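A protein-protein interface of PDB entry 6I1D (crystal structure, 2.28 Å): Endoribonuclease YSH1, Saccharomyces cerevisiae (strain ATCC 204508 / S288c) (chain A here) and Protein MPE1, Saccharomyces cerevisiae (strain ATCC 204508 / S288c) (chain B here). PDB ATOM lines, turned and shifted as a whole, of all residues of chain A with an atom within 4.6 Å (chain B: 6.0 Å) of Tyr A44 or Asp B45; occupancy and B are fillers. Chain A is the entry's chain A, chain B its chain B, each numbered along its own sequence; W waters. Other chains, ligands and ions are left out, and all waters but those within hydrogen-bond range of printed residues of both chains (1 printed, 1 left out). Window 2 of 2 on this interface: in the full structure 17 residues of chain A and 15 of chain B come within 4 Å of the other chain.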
ATOM      1  N   ARG A  22       8.194   5.527  -5.183  1.00  0.00           N
ATOM      2  CA  ARG A  22       9.527   4.974  -5.471  1.00  0.00           C
ATOM      3  C   ARG A  22      10.185   4.383  -4.220  1.00  0.00           C
ATOM      4  O   ARG A  22      11.357   4.627  -3.919  1.00  0.00           O
ATOM      5  CB  ARG A  22      10.434   6.018  -6.146  1.00  0.00           C
ATOM      6  CG  ARG A  22      10.779   7.262  -5.327  1.00  0.00           C
ATOM      7  CD  ARG A  22      11.629   8.258  -6.105  1.00  0.00           C
ATOM      8  NE  ARG A  22      11.590   9.566  -5.465  1.00  0.00           N
ATOM      9  CZ  ARG A  22      11.857  10.717  -6.074  1.00  0.00           C
ATOM     10  NH1 ARG A  22      12.202  10.734  -7.354  1.00  0.00           N
ATOM     11  NH2 ARG A  22      11.774  11.856  -5.394  1.00  0.00           N
ATOM     12  N   HIS A  41       7.961   6.229  -8.922  1.00  0.00           N
ATOM     13  CA  HIS A  41       7.171   7.396  -8.560  1.00  0.00           C
ATOM     14  C   HIS A  41       6.143   7.649  -9.650  1.00  0.00           C
ATOM     15  O   HIS A  41       6.525   8.002 -10.777  1.00  0.00           O
ATOM     16  CB  HIS A  41       8.065   8.619  -8.377  1.00  0.00           C
ATOM     17  CG  HIS A  41       7.425   9.724  -7.596  1.00  0.00           C
ATOM     18  ND1 HIS A  41       6.242  10.318  -7.979  1.00  0.00           N
ATOM     19  CD2 HIS A  41       7.806  10.346  -6.455  1.00  0.00           C
ATOM     20  CE1 HIS A  41       5.918  11.252  -7.104  1.00  0.00           C
ATOM     21  NE2 HIS A  41       6.849  11.289  -6.169  1.00  0.00           N
ATOM     22  N   PRO A  42       4.845   7.503  -9.371  1.00  0.00           N
ATOM     23  CA  PRO A  42       3.835   7.624 -10.440  1.00  0.00           C
ATOM     24  C   PRO A  42       3.795   8.988 -11.107  1.00  0.00           C
ATOM     25  O   PRO A  42       3.148   9.118 -12.155  1.00  0.00           O
ATOM     26  CB  PRO A  42       2.508   7.333  -9.721  1.00  0.00           C
ATOM     27  CG  PRO A  42       2.871   6.843  -8.360  1.00  0.00           C
ATOM     28  CD  PRO A  42       4.244   7.320  -8.043  1.00  0.00           C
ATOM     29  N   ALA A  43       4.444  10.005 -10.542  1.00  0.00           N
ATOM     30  CA  ALA A  43       4.431  11.323 -11.161  1.00  0.00           C
ATOM     31  C   ALA A  43       5.406  11.443 -12.324  1.00  0.00           C
ATOM     32  O   ALA A  43       5.337  12.428 -13.066  1.00  0.00           O
ATOM     33  CB  ALA A  43       4.738  12.401 -10.118  1.00  0.00           C
ATOM     34  N   TYR A  44       6.296  10.471 -12.512  1.00  0.00           N
ATOM     35  CA  TYR A  44       7.319  10.542 -13.542  1.00  0.00           C
ATOM     36  C   TYR A  44       7.283   9.285 -14.402  1.00  0.00           C
ATOM     37  O   TYR A  44       6.545   8.333 -14.132  1.00  0.00           O
ATOM     38  CB  TYR A  44       8.715  10.727 -12.930  1.00  0.00           C
ATOM     39  CG  TYR A  44       8.794  11.841 -11.910  1.00  0.00           C
ATOM     40  CD1 TYR A  44       8.985  13.161 -12.304  1.00  0.00           C
ATOM     41  CD2 TYR A  44       8.679  11.572 -10.552  1.00  0.00           C
ATOM     42  CE1 TYR A  44       9.057  14.184 -11.370  1.00  0.00           C
ATOM     43  CE2 TYR A  44       8.750  12.584  -9.612  1.00  0.00           C
ATOM     44  CZ  TYR A  44       8.937  13.887 -10.025  1.00  0.00           C
ATOM     45  OH  TYR A  44       9.009  14.889  -9.085  1.00  0.00           O
ATOM     46  N   GLN A  45       8.097   9.300 -15.457  1.00  0.00           N
ATOM     47  CA  GLN A  45       8.247   8.171 -16.361  1.00  0.00           C
ATOM     48  C   GLN A  45       9.726   7.943 -16.639  1.00  0.00           C
ATOM     49  O   GLN A  45      10.569   8.802 -16.373  1.00  0.00           O
ATOM     50  CB  GLN A  45       7.498   8.395 -17.680  1.00  0.00           C
ATOM     51  CG  GLN A  45       5.991   8.426 -17.543  1.00  0.00           C
ATOM     52  CD  GLN A  45       5.299   8.795 -18.841  1.00  0.00           C
ATOM     53  OE1 GLN A  45       5.950   9.125 -19.833  1.00  0.00           O
ATOM     54  NE2 GLN A  45       3.973   8.743 -18.838  1.00  0.00           N
ATOM     55  N   ALA A  48      13.427   8.858 -14.664  1.00  0.00           N
ATOM     56  CA  ALA A  48      13.012   9.873 -13.703  1.00  0.00           C
ATOM     57  C   ALA A  48      12.079   9.312 -12.635  1.00  0.00           C
ATOM     58  O   ALA A  48      11.952   9.910 -11.563  1.00  0.00           O
ATOM     59  CB  ALA A  48      12.342  11.033 -14.433  1.00  0.00           C
ATOM     60  N   SER A  49      11.427   8.181 -12.899  1.00  0.00           N
ATOM     61  CA  SER A  49      10.513   7.574 -11.942  1.00  0.00           C
ATOM     62  C   SER A  49      11.205   6.616 -10.982  1.00  0.00           C
ATOM     63  O   SER A  49      10.550   6.096 -10.073  1.00  0.00           O
ATOM     64  CB  SER A  49       9.393   6.839 -12.688  1.00  0.00           C
ATOM     65  OG  SER A  49       9.872   5.643 -13.282  1.00  0.00           O
ATOM     66  N   PHE A  52      16.821   6.388  -6.339  1.00  0.00           N
ATOM     67  CA  PHE A  52      18.160   6.911  -6.616  1.00  0.00           C
ATOM     68  C   PHE A  52      19.191   5.789  -6.465  1.00  0.00           C
ATOM     69  O   PHE A  52      20.053   5.788  -5.582  1.00  0.00           O
ATOM     70  CB  PHE A  52      18.456   8.104  -5.719  1.00  0.00           C
ATOM     71  CG  PHE A  52      17.511   9.254  -5.926  1.00  0.00           C
ATOM     72  CD1 PHE A  52      17.684  10.132  -6.987  1.00  0.00           C
ATOM     73  CD2 PHE A  52      16.435   9.447  -5.069  1.00  0.00           C
ATOM     74  CE1 PHE A  52      16.808  11.191  -7.182  1.00  0.00           C
ATOM     75  CE2 PHE A  52      15.556  10.501  -5.258  1.00  0.00           C
ATOM     76  CZ  PHE A  52      15.742  11.377  -6.314  1.00  0.00           C
ATOM     77  N   VAL A 110       6.658   1.588 -18.157  1.00  0.00           N
ATOM     78  CA  VAL A 110       6.736   2.863 -17.451  1.00  0.00           C
ATOM     79  C   VAL A 110       8.188   3.274 -17.243  1.00  0.00           C
ATOM     80  O   VAL A 110       8.537   4.455 -17.361  1.00  0.00           O
ATOM     81  CB  VAL A 110       5.972   2.781 -16.117  1.00  0.00           C
ATOM     82  CG1 VAL A 110       6.169   4.057 -15.311  1.00  0.00           C
ATOM     83  CG2 VAL A 110       4.498   2.530 -16.374  1.00  0.00           C
ATOM     84  N   LEU B  40      15.205  13.353 -17.904  1.00  0.00           N
ATOM     85  CA  LEU B  40      15.305  13.314 -16.449  1.00  0.00           C
ATOM     86  C   LEU B  40      14.444  14.358 -15.753  1.00  0.00           C
ATOM     87  O   LEU B  40      14.223  14.239 -14.542  1.00  0.00           O
ATOM     88  CB  LEU B  40      16.766  13.474 -16.023  1.00  0.00           C
ATOM     89  CG  LEU B  40      17.688  12.356 -16.513  1.00  0.00           C
ATOM     90  CD1 LEU B  40      19.096  12.524 -15.961  1.00  0.00           C
ATOM     91  CD2 LEU B  40      17.108  11.005 -16.128  1.00  0.00           C
ATOM     92  N   ASP B  42      12.919  18.601 -15.116  1.00  0.00           N
ATOM     93  CA  ASP B  42      13.307  20.003 -15.026  1.00  0.00           C
ATOM     94  C   ASP B  42      14.450  20.251 -14.051  1.00  0.00           C
ATOM     95  O   ASP B  42      14.923  21.389 -13.956  1.00  0.00           O
ATOM     96  CB  ASP B  42      12.102  20.863 -14.632  1.00  0.00           C
ATOM     97  CG  ASP B  42      11.410  20.364 -13.374  1.00  0.00           C
ATOM     98  OD1 ASP B  42      12.010  19.557 -12.631  1.00  0.00           O
ATOM     99  OD2 ASP B  42      10.259  20.784 -13.129  1.00  0.00           O
ATOM    100  N   GLY B  43      14.898  19.232 -13.321  1.00  0.00           N
ATOM    101  CA  GLY B  43      16.010  19.383 -12.412  1.00  0.00           C
ATOM    102  C   GLY B  43      15.649  19.708 -10.979  1.00  0.00           C
ATOM    103  O   GLY B  43      16.555  19.793 -10.142  1.00  0.00           O
ATOM    104  N   THR B  44      14.362  19.894 -10.663  1.00  0.00           N
ATOM    105  CA  THR B  44      13.971  20.183  -9.287  1.00  0.00           C
ATOM    106  C   THR B  44      13.962  18.944  -8.399  1.00  0.00           C
ATOM    107  O   THR B  44      13.933  19.083  -7.172  1.00  0.00           O
ATOM    108  CB  THR B  44      12.578  20.826  -9.230  1.00  0.00           C
ATOM    109  OG1 THR B  44      11.626  19.994  -9.906  1.00  0.00           O
ATOM    110  CG2 THR B  44      12.584  22.217  -9.865  1.00  0.00           C
ATOM    111  N   ASP B  45      13.978  17.745  -8.981  1.00  0.00           N
ATOM    112  CA  ASP B  45      13.850  16.506  -8.223  1.00  0.00           C
ATOM    113  C   ASP B  45      15.162  15.747  -8.077  1.00  0.00           C
ATOM    114  O   ASP B  45      15.167  14.664  -7.485  1.00  0.00           O
ATOM    115  CB  ASP B  45      12.801  15.591  -8.874  1.00  0.00           C
ATOM    116  CG  ASP B  45      12.345  14.461  -7.956  1.00  0.00           C
ATOM    117  OD1 ASP B  45      12.140  14.710  -6.749  1.00  0.00           O
ATOM    118  OD2 ASP B  45      12.193  13.320  -8.441  1.00  0.00           O
ATOM    119  N   PHE B  46      16.275  16.276  -8.577  1.00  0.00           N
ATOM    120  CA  PHE B  46      17.505  15.500  -8.550  1.00  0.00           C
ATOM    121  C   PHE B  46      18.709  16.421  -8.680  1.00  0.00           C
ATOM    122  O   PHE B  46      18.593  17.594  -9.039  1.00  0.00           O
ATOM    123  CB  PHE B  46      17.516  14.443  -9.662  1.00  0.00           C
ATOM    124  CG  PHE B  46      17.543  15.022 -11.052  1.00  0.00           C
ATOM    125  CD1 PHE B  46      16.367  15.395 -11.686  1.00  0.00           C
ATOM    126  CD2 PHE B  46      18.746  15.196 -11.722  1.00  0.00           C
ATOM    127  CE1 PHE B  46      16.390  15.932 -12.963  1.00  0.00           C
ATOM    128  CE2 PHE B  46      18.778  15.731 -13.000  1.00  0.00           C
ATOM    129  CZ  PHE B  46      17.598  16.101 -13.620  1.00  0.00           C
ATOM    130  N   GLN B  47      19.873  15.859  -8.364  1.00  0.00           N
ATOM    131  CA  GLN B  47      21.168  16.431  -8.690  1.00  0.00           C
ATOM    132  C   GLN B  47      21.881  15.489  -9.647  1.00  0.00           C
ATOM    133  O   GLN B  47      21.694  14.269  -9.593  1.00  0.00           O
ATOM    134  CB  GLN B  47      22.027  16.637  -7.439  1.00  0.00           C
ATOM    135  CG  GLN B  47      21.663  17.855  -6.613  1.00  0.00           C
ATOM    136  CD  GLN B  47      22.746  18.212  -5.616  1.00  0.00           C
ATOM    137  OE1 GLN B  47      22.913  17.542  -4.597  1.00  0.00           O
ATOM    138  NE2 GLN B  47      23.500  19.266  -5.913  1.00  0.00           N
ATOM    139  N   ARG B  76      22.883  10.158 -10.407  1.00  0.00           N
ATOM    140  CA  ARG B  76      21.688  10.957 -10.165  1.00  0.00           C
ATOM    141  C   ARG B  76      21.273  10.786  -8.706  1.00  0.00           C
ATOM    142  O   ARG B  76      20.925   9.677  -8.283  1.00  0.00           O
ATOM    143  CB  ARG B  76      20.549  10.549 -11.100  1.00  0.00           C
ATOM    144  CG  ARG B  76      19.270  11.353 -10.896  1.00  0.00           C
ATOM    145  CD  ARG B  76      18.113  10.784 -11.701  1.00  0.00           C
ATOM    146  NE  ARG B  76      17.755   9.447 -11.248  1.00  0.00           N
ATOM    147  CZ  ARG B  76      16.596   9.126 -10.683  1.00  0.00           C
ATOM    148  NH1 ARG B  76      15.661  10.046 -10.504  1.00  0.00           N
ATOM    149  NH2 ARG B  76      16.372   7.877 -10.304  1.00  0.00           N
ATOM    150  N   SER B  77      21.313  11.876  -7.947  1.00  0.00           N
ATOM    151  CA  SER B  77      21.068  11.880  -6.514  1.00  0.00           C
ATOM    152  C   SER B  77      19.870  12.765  -6.184  1.00  0.00           C
ATOM    153  O   SER B  77      19.429  13.559  -7.024  1.00  0.00           O
ATOM    154  CB  SER B  77      22.317  12.374  -5.764  1.00  0.00           C
ATOM    155  OG  SER B  77      22.673  13.689  -6.150  1.00  0.00           O
ATOM    156  N   PRO B  78      19.302  12.642  -4.979  1.00  0.00           N
ATOM    157  CA  PRO B  78      18.178  13.514  -4.611  1.00  0.00           C
ATOM    158  C   PRO B  78      18.589  14.976  -4.568  1.00  0.00           C
ATOM    159  O   PRO B  78      19.746  15.314  -4.307  1.00  0.00           O
ATOM    160  CB  PRO B  78      17.775  13.018  -3.214  1.00  0.00           C
ATOM    161  CG  PRO B  78      18.352  11.656  -3.095  1.00  0.00           C
ATOM    162  CD  PRO B  78      19.587  11.641  -3.935  1.00  0.00           C
ATOM    163  N   ALA B  79      17.618  15.848  -4.824  1.00  0.00           N
ATOM    164  CA  ALA B  79      17.835  17.274  -4.637  1.00  0.00           C
ATOM    165  C   ALA B  79      17.917  17.594  -3.149  1.00  0.00           C
ATOM    166  O   ALA B  79      17.152  17.063  -2.340  1.00  0.00           O
ATOM    167  CB  ALA B  79      16.711  18.078  -5.289  1.00  0.00           C
ATOM    168  N   ASN B 100      20.327  21.476  -6.830  1.00  0.00           N
ATOM    169  CA  ASN B 100      19.542  20.675  -7.761  1.00  0.00           C
ATOM    170  C   ASN B 100      20.202  20.774  -9.132  1.00  0.00           C
ATOM    171  O   ASN B 100      21.363  21.179  -9.247  1.00  0.00           O
ATOM    172  CB  ASN B 100      18.068  21.123  -7.754  1.00  0.00           C
ATOM    173  CG  ASN B 100      17.893  22.597  -8.078  1.00  0.00           C
ATOM    174  OD1 ASN B 100      18.732  23.212  -8.735  1.00  0.00           O
ATOM    175  ND2 ASN B 100      16.796  23.173  -7.606  1.00  0.00           N
HETATM  176  O   HOH W   1      12.538  12.574 -10.987  1.00  0.00           O
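The guanidinium group (NH1) of Arg A22 lies within salt-bridge range of the side-chain carboxylate (OD2) of Asp B45 (2.8 Å).
The backbone NH (N) of Gln B47 sits at hydrogen-bond distance from the backbone carbonyl oxygen (O) of Ser B77 (2.7 Å).
Among the printed residues, merely in contact across the chains: Phe A52 with Ser B77, Phe A52 with Arg B76, Phe A52 with Pro B78, Phe A52 with Asp B45, Tyr A44 with Asp B45, Ala A48 with Leu B40 and Ala A48 with Arg B76.
Tyr A44 touches just one residue of chain B: Asp B45.
Asp B45 touches three residues of chain A.
Of the printed residues of chain B, Ala A48 touches Leu B40 (3.7 Å) and Arg B76 (3.9 Å).
Printed residues of chain A within 4 Å of Pro B78: Phe A52 (3.5 Å).
Of the printed residues of chain B, Phe A52 touches Asp B45 (3.5 Å), Arg B76 (3.5 Å), Ser B77 (3.5 Å) and Pro B78 (3.5 Å).
Printed residues of chain A within 4 Å of Leu B40: Ala A48 (3.7 Å).
The nearest printed residue of chain B that does not touch Tyr A44 is Thr B44 (5.8 Å).
Of the 12 printed residues of chain B, 5 touch a printed residue of chain A.
Hydrophobic or aromatic side chains of chain B within 4 Å of the printed part of chain A: Pro B78.
Hydrophobic or aromatic side chains of chain A within 4 Å of the printed part of chain B: Tyr A44, Ala A48 and Phe A52.
Along chain A the printed residues that touch a printed residue of chain B span positions 22 to 52.
Among the printed residues, 8 pairs touch across the chains.
Among the printed residues, Asp or Glu carboxylates within 4 Å of a Lys or Arg side-chain nitrogen of the other chain: Arg A22 with Asp B45 (2.8 Å).
Water W1 bridges OD2 of Asp B45 and O of Ala A48.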
